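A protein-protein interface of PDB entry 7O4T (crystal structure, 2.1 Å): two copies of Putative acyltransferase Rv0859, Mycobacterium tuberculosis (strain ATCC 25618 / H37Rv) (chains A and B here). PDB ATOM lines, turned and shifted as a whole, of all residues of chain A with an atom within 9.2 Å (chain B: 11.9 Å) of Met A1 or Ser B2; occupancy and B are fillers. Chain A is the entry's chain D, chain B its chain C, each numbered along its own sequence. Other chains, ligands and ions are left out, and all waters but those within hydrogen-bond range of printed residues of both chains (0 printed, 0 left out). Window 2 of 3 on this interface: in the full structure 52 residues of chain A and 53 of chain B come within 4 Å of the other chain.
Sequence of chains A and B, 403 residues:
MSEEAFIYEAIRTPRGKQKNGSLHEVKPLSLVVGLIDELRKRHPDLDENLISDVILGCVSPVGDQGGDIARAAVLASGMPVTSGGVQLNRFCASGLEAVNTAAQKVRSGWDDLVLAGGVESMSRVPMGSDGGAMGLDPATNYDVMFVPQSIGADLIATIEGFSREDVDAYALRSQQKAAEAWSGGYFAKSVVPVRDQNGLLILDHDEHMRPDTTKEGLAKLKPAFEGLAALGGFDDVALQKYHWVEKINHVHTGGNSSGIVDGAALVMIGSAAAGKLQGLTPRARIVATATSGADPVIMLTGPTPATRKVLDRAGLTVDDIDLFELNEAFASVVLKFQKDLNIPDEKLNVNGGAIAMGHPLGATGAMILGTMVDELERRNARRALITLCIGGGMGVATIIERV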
ATOM      1  N   MET A   1      27.604 -33.289   8.350  1.00  0.00           N
ATOM      2  CA  MET A   1      27.502 -34.446   9.230  1.00  0.00           C
ATOM      3  C   MET A   1      28.728 -34.548  10.132  1.00  0.00           C
ATOM      4  O   MET A   1      29.209 -35.643  10.427  1.00  0.00           O
ATOM      5  CB  MET A   1      27.333 -35.731   8.414  1.00  0.00           C
ATOM      6  N   SER A   2      29.223 -33.393  10.576  1.00  0.00           N
ATOM      7  CA  SER A   2      30.442 -33.338  11.371  1.00  0.00           C
ATOM      8  C   SER A   2      30.150 -32.952  12.816  1.00  0.00           C
ATOM      9  O   SER A   2      30.063 -33.820  13.690  1.00  0.00           O
ATOM     10  CB  SER A   2      31.434 -32.351  10.748  1.00  0.00           C
ATOM     11  OG  SER A   2      32.596 -32.211  11.550  1.00  0.00           O
ATOM     12  N   GLU A   3      30.002 -31.654  13.074  1.00  0.00           N
ATOM     13  CA  GLU A   3      29.832 -31.166  14.436  1.00  0.00           C
ATOM     14  C   GLU A   3      28.521 -31.665  15.031  1.00  0.00           C
ATOM     15  O   GLU A   3      27.451 -31.469  14.451  1.00  0.00           O
ATOM     16  CB  GLU A   3      29.861 -29.638  14.461  1.00  0.00           C
ATOM     17  CG  GLU A   3      31.248 -29.020  14.386  1.00  0.00           C
ATOM     18  CD  GLU A   3      31.911 -28.896  15.747  1.00  0.00           C
ATOM     19  OE1 GLU A   3      31.695 -29.777  16.605  1.00  0.00           O
ATOM     20  OE2 GLU A   3      32.642 -27.906  15.961  1.00  0.00           O
ATOM     21  N   GLU A   4      28.606 -32.305  16.193  1.00  0.00           N
ATOM     22  CA  GLU A   4      27.402 -32.705  16.905  1.00  0.00           C
ATOM     23  C   GLU A   4      26.681 -31.478  17.451  1.00  0.00           C
ATOM     24  O   GLU A   4      27.303 -30.484  17.840  1.00  0.00           O
ATOM     25  CB  GLU A   4      27.747 -33.668  18.042  1.00  0.00           C
ATOM     26  CG  GLU A   4      28.355 -34.984  17.580  1.00  0.00           C
ATOM     27  CD  GLU A   4      27.368 -35.849  16.818  1.00  0.00           C
ATOM     28  OE1 GLU A   4      26.152 -35.760  17.095  1.00  0.00           O
ATOM     29  OE2 GLU A   4      27.810 -36.618  15.938  1.00  0.00           O
ATOM     30  N   ALA A   5      25.353 -31.549  17.468  1.00  0.00           N
ATOM     31  CA  ALA A   5      24.510 -30.463  17.950  1.00  0.00           C
ATOM     32  C   ALA A   5      23.894 -30.857  19.286  1.00  0.00           C
ATOM     33  O   ALA A   5      23.312 -31.939  19.409  1.00  0.00           O
ATOM     34  CB  ALA A   5      23.413 -30.124  16.936  1.00  0.00           C
ATOM     35  N   ALA A 103      19.819 -27.262  14.490  1.00  0.00           N
ATOM     36  CA  ALA A 103      20.736 -28.384  14.660  1.00  0.00           C
ATOM     37  C   ALA A 103      21.530 -28.641  13.387  1.00  0.00           C
ATOM     38  O   ALA A 103      22.727 -28.949  13.444  1.00  0.00           O
ATOM     39  CB  ALA A 103      19.966 -29.637  15.073  1.00  0.00           C
ATOM     40  N   GLN A 104      20.884 -28.515  12.226  1.00  0.00           N
ATOM     41  CA  GLN A 104      21.589 -28.734  10.968  1.00  0.00           C
ATOM     42  C   GLN A 104      22.575 -27.608  10.682  1.00  0.00           C
ATOM     43  O   GLN A 104      23.652 -27.849  10.125  1.00  0.00           O
ATOM     44  CB  GLN A 104      20.585 -28.888   9.827  1.00  0.00           C
ATOM     45  CG  GLN A 104      19.839 -30.214   9.860  1.00  0.00           C
ATOM     46  CD  GLN A 104      18.609 -30.223   8.973  1.00  0.00           C
ATOM     47  OE1 GLN A 104      17.807 -29.288   8.992  1.00  0.00           O
ATOM     48  NE2 GLN A 104      18.453 -31.285   8.188  1.00  0.00           N
ATOM     49  N   LYS A 105      22.229 -26.373  11.059  1.00  0.00           N
ATOM     50  CA  LYS A 105      23.167 -25.266  10.903  1.00  0.00           C
ATOM     51  C   LYS A 105      24.424 -25.487  11.735  1.00  0.00           C
ATOM     52  O   LYS A 105      25.536 -25.186  11.286  1.00  0.00           O
ATOM     53  CB  LYS A 105      22.499 -23.945  11.285  1.00  0.00           C
ATOM     54  CG  LYS A 105      21.577 -23.375  10.218  1.00  0.00           C
ATOM     55  CD  LYS A 105      20.941 -22.075  10.685  1.00  0.00           C
ATOM     56  CE  LYS A 105      20.037 -21.470   9.617  1.00  0.00           C
ATOM     57  NZ  LYS A 105      20.804 -21.043   8.412  1.00  0.00           N
ATOM     58  N   VAL A 106      24.265 -26.013  12.953  1.00  0.00           N
ATOM     59  CA  VAL A 106      25.423 -26.306  13.793  1.00  0.00           C
ATOM     60  C   VAL A 106      26.241 -27.443  13.196  1.00  0.00           C
ATOM     61  O   VAL A 106      27.478 -27.392  13.176  1.00  0.00           O
ATOM     62  CB  VAL A 106      24.973 -26.627  15.230  1.00  0.00           C
ATOM     63  CG1 VAL A 106      26.133 -27.201  16.042  1.00  0.00           C
ATOM     64  CG2 VAL A 106      24.420 -25.384  15.897  1.00  0.00           C
ATOM     65  N   ARG A 107      25.569 -28.482  12.693  1.00  0.00           N
ATOM     66  CA  ARG A 107      26.282 -29.631  12.144  1.00  0.00           C
ATOM     67  C   ARG A 107      27.079 -29.267  10.900  1.00  0.00           C
ATOM     68  O   ARG A 107      28.116 -29.884  10.629  1.00  0.00           O
ATOM     69  CB  ARG A 107      25.302 -30.756  11.826  1.00  0.00           C
ATOM     70  CG  ARG A 107      24.717 -31.411  13.055  1.00  0.00           C
ATOM     71  CD  ARG A 107      23.673 -32.429  12.683  1.00  0.00           C
ATOM     72  NE  ARG A 107      24.185 -33.457  11.781  1.00  0.00           N
ATOM     73  CZ  ARG A 107      24.807 -34.560  12.183  1.00  0.00           C
ATOM     74  NH1 ARG A 107      25.006 -34.779  13.476  1.00  0.00           N
ATOM     75  NH2 ARG A 107      25.229 -35.445  11.291  1.00  0.00           N
ATOM     76  N   SER A 108      26.613 -28.282  10.129  1.00  0.00           N
ATOM     77  CA  SER A 108      27.342 -27.861   8.939  1.00  0.00           C
ATOM     78  C   SER A 108      28.637 -27.137   9.279  1.00  0.00           C
ATOM     79  O   SER A 108      29.494 -26.984   8.402  1.00  0.00           O
ATOM     80  CB  SER A 108      26.462 -26.959   8.073  1.00  0.00           C
ATOM     81  OG  SER A 108      26.291 -25.689   8.678  1.00  0.00           O
ATOM     82  N   GLY A 109      28.796 -26.685  10.523  1.00  0.00           N
ATOM     83  CA  GLY A 109      29.981 -25.971  10.943  1.00  0.00           C
ATOM     84  C   GLY A 109      29.941 -24.474  10.725  1.00  0.00           C
ATOM     85  O   GLY A 109      30.822 -23.767  11.230  1.00  0.00           O
ATOM     86  N   TRP A 110      28.948 -23.967   9.999  1.00  0.00           N
ATOM     87  CA  TRP A 110      28.869 -22.552   9.667  1.00  0.00           C
ATOM     88  C   TRP A 110      28.019 -21.759  10.653  1.00  0.00           C
ATOM     89  O   TRP A 110      27.707 -20.593  10.391  1.00  0.00           O
ATOM     90  CB  TRP A 110      28.346 -22.391   8.237  1.00  0.00           C
ATOM     91  CG  TRP A 110      29.264 -23.033   7.231  1.00  0.00           C
ATOM     92  CD1 TRP A 110      30.584 -23.337   7.409  1.00  0.00           C
ATOM     93  CD2 TRP A 110      28.929 -23.471   5.909  1.00  0.00           C
ATOM     94  NE1 TRP A 110      31.094 -23.922   6.278  1.00  0.00           N
ATOM     95  CE2 TRP A 110      30.098 -24.018   5.342  1.00  0.00           C
ATOM     96  CE3 TRP A 110      27.757 -23.451   5.147  1.00  0.00           C
ATOM     97  CZ2 TRP A 110      30.129 -24.540   4.052  1.00  0.00           C
ATOM     98  CZ3 TRP A 110      27.791 -23.967   3.865  1.00  0.00           C
ATOM     99  CH2 TRP A 110      28.970 -24.499   3.329  1.00  0.00           C
ATOM    100  N   VAL A 287      20.263 -36.567  17.670  1.00  0.00           N
ATOM    101  CA  VAL A 287      20.835 -37.743  17.021  1.00  0.00           C
ATOM    102  C   VAL A 287      20.536 -37.745  15.529  1.00  0.00           C
ATOM    103  O   VAL A 287      21.422 -38.023  14.711  1.00  0.00           O
ATOM    104  CB  VAL A 287      20.323 -39.025  17.701  1.00  0.00           C
ATOM    105  CG1 VAL A 287      20.913 -40.257  17.025  1.00  0.00           C
ATOM    106  CG2 VAL A 287      20.661 -39.006  19.184  1.00  0.00           C
ATOM    107  N   SER B   2      30.707 -32.131   6.448  1.00  0.00           N
ATOM    108  CA  SER B   2      31.024 -33.448   5.908  1.00  0.00           C
ATOM    109  C   SER B   2      30.695 -33.520   4.419  1.00  0.00           C
ATOM    110  O   SER B   2      31.576 -33.374   3.572  1.00  0.00           O
ATOM    111  CB  SER B   2      30.268 -34.537   6.672  1.00  0.00           C
ATOM    112  OG  SER B   2      30.584 -35.827   6.178  1.00  0.00           O
ATOM    113  N   GLU B   3      29.422 -33.753   4.109  1.00  0.00           N
ATOM    114  CA  GLU B   3      28.986 -33.798   2.721  1.00  0.00           C
ATOM    115  C   GLU B   3      29.115 -32.422   2.079  1.00  0.00           C
ATOM    116  O   GLU B   3      28.865 -31.397   2.718  1.00  0.00           O
ATOM    117  CB  GLU B   3      27.536 -34.278   2.634  1.00  0.00           C
ATOM    118  CG  GLU B   3      27.311 -35.713   3.082  1.00  0.00           C
ATOM    119  CD  GLU B   3      27.472 -36.713   1.954  1.00  0.00           C
ATOM    120  OE1 GLU B   3      27.990 -36.329   0.883  1.00  0.00           O
ATOM    121  OE2 GLU B   3      27.070 -37.882   2.134  1.00  0.00           O
ATOM    122  N   GLU B   4      29.510 -32.401   0.810  1.00  0.00           N
ATOM    123  CA  GLU B   4      29.590 -31.158   0.058  1.00  0.00           C
ATOM    124  C   GLU B   4      28.260 -30.880  -0.628  1.00  0.00           C
ATOM    125  O   GLU B   4      27.589 -31.799  -1.109  1.00  0.00           O
ATOM    126  CB  GLU B   4      30.716 -31.214  -0.978  1.00  0.00           C
ATOM    127  CG  GLU B   4      32.118 -31.216  -0.380  1.00  0.00           C
ATOM    128  CD  GLU B   4      32.468 -29.910   0.313  1.00  0.00           C
ATOM    129  OE1 GLU B   4      31.918 -28.859  -0.079  1.00  0.00           O
ATOM    130  OE2 GLU B   4      33.293 -29.933   1.251  1.00  0.00           O
ATOM    131  N   ALA B   5      27.879 -29.606  -0.664  1.00  0.00           N
ATOM    132  CA  ALA B   5      26.619 -29.176  -1.255  1.00  0.00           C
ATOM    133  C   ALA B   5      26.892 -28.583  -2.632  1.00  0.00           C
ATOM    134  O   ALA B   5      27.675 -27.636  -2.760  1.00  0.00           O
ATOM    135  CB  ALA B   5      25.915 -28.161  -0.356  1.00  0.00           C
ATOM    136  N   PHE B   6      26.242 -29.136  -3.653  1.00  0.00           N
ATOM    137  CA  PHE B   6      26.444 -28.720  -5.034  1.00  0.00           C
ATOM    138  C   PHE B   6      25.156 -28.141  -5.603  1.00  0.00           C
ATOM    139  O   PHE B   6      24.057 -28.600  -5.278  1.00  0.00           O
ATOM    140  CB  PHE B   6      26.910 -29.898  -5.901  1.00  0.00           C
ATOM    141  CG  PHE B   6      28.251 -30.454  -5.503  1.00  0.00           C
ATOM    142  CD1 PHE B   6      29.420 -29.911  -6.010  1.00  0.00           C
ATOM    143  CD2 PHE B   6      28.341 -31.520  -4.623  1.00  0.00           C
ATOM    144  CE1 PHE B   6      30.656 -30.419  -5.649  1.00  0.00           C
ATOM    145  CE2 PHE B   6      29.574 -32.034  -4.257  1.00  0.00           C
ATOM    146  CZ  PHE B   6      30.733 -31.481  -4.772  1.00  0.00           C
ATOM    147  N   THR B 101      20.284 -22.409   3.731  1.00  0.00           N
ATOM    148  CA  THR B 101      19.693 -23.434   4.585  1.00  0.00           C
ATOM    149  C   THR B 101      19.645 -24.778   3.871  1.00  0.00           C
ATOM    150  O   THR B 101      19.920 -25.820   4.475  1.00  0.00           O
ATOM    151  CB  THR B 101      18.292 -23.009   5.031  1.00  0.00           C
ATOM    152  OG1 THR B 101      18.381 -21.815   5.816  1.00  0.00           O
ATOM    153  CG2 THR B 101      17.639 -24.099   5.866  1.00  0.00           C
ATOM    154  N   ALA B 102      19.313 -24.771   2.579  1.00  0.00           N
ATOM    155  CA  ALA B 102      19.326 -26.010   1.807  1.00  0.00           C
ATOM    156  C   ALA B 102      20.716 -26.632   1.787  1.00  0.00           C
ATOM    157  O   ALA B 102      20.859 -27.854   1.903  1.00  0.00           O
ATOM    158  CB  ALA B 102      18.839 -25.747   0.385  1.00  0.00           C
ATOM    159  N   ALA B 103      21.754 -25.805   1.638  1.00  0.00           N
ATOM    160  CA  ALA B 103      23.117 -26.328   1.622  1.00  0.00           C
ATOM    161  C   ALA B 103      23.498 -26.920   2.973  1.00  0.00           C
ATOM    162  O   ALA B 103      24.120 -27.986   3.035  1.00  0.00           O
ATOM    163  CB  ALA B 103      24.100 -25.225   1.223  1.00  0.00           C
ATOM    164  N   GLN B 104      23.128 -26.244   4.064  1.00  0.00           N
ATOM    165  CA  GLN B 104      23.478 -26.736   5.393  1.00  0.00           C
ATOM    166  C   GLN B 104      22.751 -28.036   5.712  1.00  0.00           C
ATOM    167  O   GLN B 104      23.313 -28.919   6.370  1.00  0.00           O
ATOM    168  CB  GLN B 104      23.177 -25.667   6.442  1.00  0.00           C
ATOM    169  CG  GLN B 104      24.112 -24.471   6.372  1.00  0.00           C
ATOM    170  CD  GLN B 104      23.579 -23.258   7.113  1.00  0.00           C
ATOM    171  OE1 GLN B 104      22.446 -22.827   6.891  1.00  0.00           O
ATOM    172  NE2 GLN B 104      24.396 -22.703   8.001  1.00  0.00           N
ATOM    173  N   LYS B 105      21.501 -28.173   5.258  1.00  0.00           N
ATOM    174  CA  LYS B 105      20.790 -29.437   5.430  1.00  0.00           C
ATOM    175  C   LYS B 105      21.471 -30.556   4.653  1.00  0.00           C
ATOM    176  O   LYS B 105      21.554 -31.694   5.131  1.00  0.00           O
ATOM    177  CB  LYS B 105      19.331 -29.291   4.992  1.00  0.00           C
ATOM    178  CG  LYS B 105      18.517 -28.324   5.833  1.00  0.00           C
ATOM    179  CD  LYS B 105      17.203 -27.963   5.154  1.00  0.00           C
ATOM    180  CE  LYS B 105      16.035 -28.759   5.714  1.00  0.00           C
ATOM    181  NZ  LYS B 105      15.715 -28.353   7.112  1.00  0.00           N
ATOM    182  N   VAL B 106      21.959 -30.254   3.448  1.00  0.00           N
ATOM    183  CA  VAL B 106      22.692 -31.251   2.673  1.00  0.00           C
ATOM    184  C   VAL B 106      23.987 -31.627   3.380  1.00  0.00           C
ATOM    185  O   VAL B 106      24.345 -32.809   3.467  1.00  0.00           O
ATOM    186  CB  VAL B 106      22.954 -30.732   1.246  1.00  0.00           C
ATOM    187  CG1 VAL B 106      23.956 -31.624   0.526  1.00  0.00           C
ATOM    188  CG2 VAL B 106      21.653 -30.656   0.464  1.00  0.00           C
ATOM    189  N   ARG B 107      24.706 -30.630   3.906  1.00  0.00           N
ATOM    190  CA  ARG B 107      25.964 -30.901   4.594  1.00  0.00           C
ATOM    191  C   ARG B 107      25.754 -31.733   5.851  1.00  0.00           C
ATOM    192  O   ARG B 107      26.606 -32.560   6.193  1.00  0.00           O
ATOM    193  CB  ARG B 107      26.668 -29.590   4.945  1.00  0.00           C
ATOM    194  CG  ARG B 107      27.298 -28.887   3.758  1.00  0.00           C
ATOM    195  CD  ARG B 107      27.952 -27.583   4.171  1.00  0.00           C
ATOM    196  NE  ARG B 107      28.980 -27.760   5.193  1.00  0.00           N
ATOM    197  CZ  ARG B 107      30.276 -27.910   4.936  1.00  0.00           C
ATOM    198  NH1 ARG B 107      30.712 -27.909   3.685  1.00  0.00           N
ATOM    199  NH2 ARG B 107      31.138 -28.060   5.931  1.00  0.00           N
ATOM    200  N   SER B 108      24.633 -31.534   6.548  1.00  0.00           N
ATOM    201  CA  SER B 108      24.361 -32.298   7.760  1.00  0.00           C
ATOM    202  C   SER B 108      24.149 -33.779   7.478  1.00  0.00           C
ATOM    203  O   SER B 108      24.222 -34.589   8.408  1.00  0.00           O
ATOM    204  CB  SER B 108      23.135 -31.734   8.480  1.00  0.00           C
ATOM    205  OG  SER B 108      21.943 -32.093   7.800  1.00  0.00           O
ATOM    206  N   GLY B 109      23.885 -34.148   6.225  1.00  0.00           N
ATOM    207  CA  GLY B 109      23.668 -35.528   5.856  1.00  0.00           C
ATOM    208  C   GLY B 109      22.237 -36.003   5.973  1.00  0.00           C
ATOM    209  O   GLY B 109      21.916 -37.084   5.462  1.00  0.00           O
ATOM    210  N   TRP B 110      21.366 -35.233   6.619  1.00  0.00           N
ATOM    211  CA  TRP B 110      19.983 -35.629   6.838  1.00  0.00           C
ATOM    212  C   TRP B 110      19.054 -35.152   5.729  1.00  0.00           C
ATOM    213  O   TRP B 110      17.830 -35.204   5.893  1.00  0.00           O
ATOM    214  CB  TRP B 110      19.515 -35.117   8.201  1.00  0.00           C
ATOM    215  CG  TRP B 110      20.339 -35.676   9.326  1.00  0.00           C
ATOM    216  CD1 TRP B 110      21.092 -36.814   9.298  1.00  0.00           C
ATOM    217  CD2 TRP B 110      20.511 -35.115  10.634  1.00  0.00           C
ATOM    218  NE1 TRP B 110      21.713 -37.003  10.507  1.00  0.00           N
ATOM    219  CE2 TRP B 110      21.374 -35.973  11.345  1.00  0.00           C
ATOM    220  CE3 TRP B 110      20.020 -33.973  11.273  1.00  0.00           C
ATOM    221  CZ2 TRP B 110      21.753 -35.726  12.662  1.00  0.00           C
ATOM    222  CZ3 TRP B 110      20.397 -33.731  12.581  1.00  0.00           C
ATOM    223  CH2 TRP B 110      21.249 -34.607  13.263  1.00  0.00           C
ATOM    224  N   ASP B 111      19.611 -34.696   4.609  1.00  0.00           N
ATOM    225  CA  ASP B 111      18.845 -34.305   3.435  1.00  0.00           C
ATOM    226  C   ASP B 111      19.712 -34.546   2.208  1.00  0.00           C
ATOM    227  O   ASP B 111      20.903 -34.227   2.211  1.00  0.00           O
ATOM    228  CB  ASP B 111      18.401 -32.838   3.509  1.00  0.00           C
ATOM    229  CG  ASP B 111      17.131 -32.653   4.324  1.00  0.00           C
ATOM    230  OD1 ASP B 111      16.115 -33.298   3.992  1.00  0.00           O
ATOM    231  OD2 ASP B 111      17.149 -31.873   5.301  1.00  0.00           O
ATOM    232  N   ASP B 112      19.109 -35.112   1.164  1.00  0.00           N
ATOM    233  CA  ASP B 112      19.841 -35.524  -0.029  1.00  0.00           C
ATOM    234  C   ASP B 112      19.697 -34.539  -1.183  1.00  0.00           C
ATOM    235  O   ASP B 112      20.702 -34.096  -1.747  1.00  0.00           O
ATOM    236  CB  ASP B 112      19.374 -36.915  -0.473  1.00  0.00           C
ATOM    237  CG  ASP B 112      19.668 -37.985   0.561  1.00  0.00           C
ATOM    238  OD1 ASP B 112      20.840 -38.106   0.978  1.00  0.00           O
ATOM    239  OD2 ASP B 112      18.725 -38.700   0.962  1.00  0.00           O
ATOM    240  N   GLY B 270      22.058 -30.406  -3.905  1.00  0.00           N
ATOM    241  CA  GLY B 270      22.167 -31.781  -3.452  1.00  0.00           C
ATOM    242  C   GLY B 270      23.604 -32.186  -3.223  1.00  0.00           C
ATOM    243  O   GLY B 270      24.545 -31.454  -3.536  1.00  0.00           O
ATOM    244  N   SER B 271      23.755 -33.380  -2.657  1.00  0.00           N
ATOM    245  CA  SER B 271      25.065 -33.968  -2.443  1.00  0.00           C
ATOM    246  C   SER B 271      25.577 -34.598  -3.735  1.00  0.00           C
ATOM    247  O   SER B 271      24.847 -34.753  -4.718  1.00  0.00           O
ATOM    248  CB  SER B 271      25.006 -35.013  -1.331  1.00  0.00           C
ATOM    249  OG  SER B 271      24.088 -36.043  -1.656  1.00  0.00           O
ATOM    250  N   ALA B 272      26.860 -34.966  -3.723  1.00  0.00           N
ATOM    251  CA  ALA B 272      27.448 -35.615  -4.890  1.00  0.00           C
ATOM    252  C   ALA B 272      26.779 -36.953  -5.168  1.00  0.00           C
ATOM    253  O   ALA B 272      26.523 -37.298  -6.329  1.00  0.00           O
ATOM    254  CB  ALA B 272      28.953 -35.797  -4.689  1.00  0.00           C
ATOM    255  N   ALA B 273      26.482 -37.718  -4.114  1.00  0.00           N
ATOM    256  CA  ALA B 273      25.818 -39.004  -4.297  1.00  0.00           C
ATOM    257  C   ALA B 273      24.412 -38.824  -4.849  1.00  0.00           C
ATOM    258  O   ALA B 273      23.967 -39.604  -5.700  1.00  0.00           O
ATOM    259  CB  ALA B 273      25.781 -39.768  -2.973  1.00  0.00           C
ATOM    260  N   ARG B 285      29.750 -25.449  -6.450  1.00  0.00           N
ATOM    261  CA  ARG B 285      29.817 -25.967  -5.093  1.00  0.00           C
ATOM    262  C   ARG B 285      29.644 -24.822  -4.104  1.00  0.00           C
ATOM    263  O   ARG B 285      30.225 -23.748  -4.281  1.00  0.00           O
ATOM    264  CB  ARG B 285      31.156 -26.680  -4.843  1.00  0.00           C
ATOM    265  CG  ARG B 285      31.307 -27.283  -3.451  1.00  0.00           C
ATOM    266  CD  ARG B 285      32.642 -28.008  -3.293  1.00  0.00           C
ATOM    267  NE  ARG B 285      33.777 -27.087  -3.272  1.00  0.00           N
ATOM    268  CZ  ARG B 285      34.304 -26.579  -2.162  1.00  0.00           C
ATOM    269  NH1 ARG B 285      33.801 -26.902  -0.978  1.00  0.00           N
ATOM    270  NH2 ARG B 285      35.335 -25.747  -2.234  1.00  0.00           N
ATOM    271  N   ILE B 286      28.842 -25.050  -3.067  1.00  0.00           N
ATOM    272  CA  ILE B 286      28.685 -24.070  -1.995  1.00  0.00           C
ATOM    273  C   ILE B 286      29.907 -24.177  -1.090  1.00  0.00           C
ATOM    274  O   ILE B 286      30.093 -25.183  -0.403  1.00  0.00           O
ATOM    275  CB  ILE B 286      27.389 -24.292  -1.207  1.00  0.00           C
ATOM    276  CG1 ILE B 286      26.183 -24.328  -2.146  1.00  0.00           C
ATOM    277  CG2 ILE B 286      27.215 -23.198  -0.160  1.00  0.00           C
ATOM    278  CD1 ILE B 286      25.795 -22.980  -2.680  1.00  0.00           C
ATOM    279  N   VAL B 287      30.748 -23.142  -1.092  1.00  0.00           N
ATOM    280  CA  VAL B 287      31.997 -23.195  -0.338  1.00  0.00           C
ATOM    281  C   VAL B 287      31.766 -22.830   1.122  1.00  0.00           C
ATOM    282  O   VAL B 287      32.269 -23.502   2.031  1.00  0.00           O
ATOM    283  CB  VAL B 287      33.056 -22.284  -0.986  1.00  0.00           C
ATOM    284  CG1 VAL B 287      34.334 -22.280  -0.163  1.00  0.00           C
ATOM    285  CG2 VAL B 287      33.344 -22.740  -2.398  1.00  0.00           C
ATOM    286  N   ALA B 288      31.005 -21.766   1.370  1.00  0.00           N
ATOM    287  CA  ALA B 288      30.767 -21.313   2.733  1.00  0.00           C
ATOM    288  C   ALA B 288      29.586 -20.353   2.751  1.00  0.00           C
ATOM    289  O   ALA B 288      29.283 -19.701   1.750  1.00  0.00           O
ATOM    290  CB  ALA B 288      32.009 -20.634   3.322  1.00  0.00           C
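The side-chain amino group of Lys A105 is in hydrogen-bond range of the side-chain amide oxygen of Gln B104 (2.9 Å).
N of Met A1 is in hydrogen-bond range of O of Arg B107 (2.5 Å).
The backbone carbonyl oxygen (O) of Ser A108 sits at hydrogen-bond distance from the guanidinium group (NH2) of Arg B107 (3.2 Å).
NZ of Lys B105 is in hydrogen-bond range of OE1 of Gln A104, 3.0 Å away.
O of Ser B108 is in hydrogen-bond range of NH2 of Arg A107, 3.2 Å away.
The side-chain carboxylate (OD2) of Asp B111 lies within hydrogen-bond range of the side-chain amide nitrogen (NE2) of Gln A104.
OG of Ser B108 sits close to N of Trp B110, at 3.4 Å.
The backbone carbonyl oxygen of Lys B105 is in hydrogen-bond range of the side-chain hydroxyl of Ser B108, 2.7 Å away.
The side-chain carboxylate (OE1) of Glu A4 lies within salt-bridge range of the guanidinium group (NH1) of Arg A107 (3.9 Å).
O of Lys A105 is in hydrogen-bond range of OG of Ser A108, at 2.8 Å.
The backbone NH (N) of Trp A110 sits close to the side-chain hydroxyl (OG) of Ser A108.
The backbone carbonyl oxygen (O) of Ala B5 lies within hydrogen-bond range of the backbone NH (N) of Ile B286 (2.9 Å).
Ser B2 touches Met A1 (CB to N, 3.4 Å).
CB of Met A1 touches O of Ser B108 (3.3 Å).
O of Gln A104 touches O of Gln B104, at 3.9 Å.
Ser B108 touches Gln A104 (OG to CG, 3.5 Å).
Lys A105 touches Thr B101 (NZ to OG1, 3.6 Å).
Arg A107 touches Trp B110.
OG of Ser A108 touches CG of Gln B104 (3.4 Å).
Trp A110 touches Arg B107.
Trp A110 touches Ile B286 (CH2 to O, 3.96 Å).
O of Val B287 touches CZ2 of Trp A110 (3.1 Å).
Of chain B, only Ser B2, Arg B107 and Ser B108 come within 4 Å of Met A1.
Arg A107 touches just these residues of chain B: Ser B108 and Trp B110.
Ser B2 touches just one residue of chain A: Met A1.
Of the printed residues of chain A, Lys B105 touches Gln A104 (3.0 Å).
Of the printed residues of chain A, Trp B110 touches Gln A104 (3.98 Å), Arg A107 (3.3 Å) and Val A287 (3.1 Å).
Ser B271 touches none of the printed residues of chain A.
Of the printed residues of chain A, Ala B288 touches Trp A110 (3.5 Å).
The nearest residue of chain B that does not touch Met A1 is Gly B109 (4.4 Å).
The nearest printed residue of chain A that does not touch Ser B108 is Ser A108 (5.2 Å).
Printed residues of chain A that touch a printed residue of chain B: Met A1, Gln A104, Lys A105, Arg A107, Ser A108, Trp A110 and Val A287.
Of the 25 printed residues of chain B, 11 touch a printed residue of chain A.
Among the printed residues, 20 pairs touch across the chains.
Among the printed residues, no Asp or Glu carboxylate lies within 4 Å of a Lys or Arg side-chain nitrogen of the other chain.
Gln A104 touches its own counterpart, Gln B104.
Gln A104 touches Lys B105, and with the chains exchanged Lys A105 touches Gln B104.
Gln A104 touches Ser B108, and with the chains exchanged Ser A108 touches Gln B104.
Arg A107 touches Trp B110, and with the chains exchanged Trp A110 touches Arg B107.
Of the 20 pairs that touch across the chains among the printed residues, 13 have their exchanged pair printed and touching as well.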
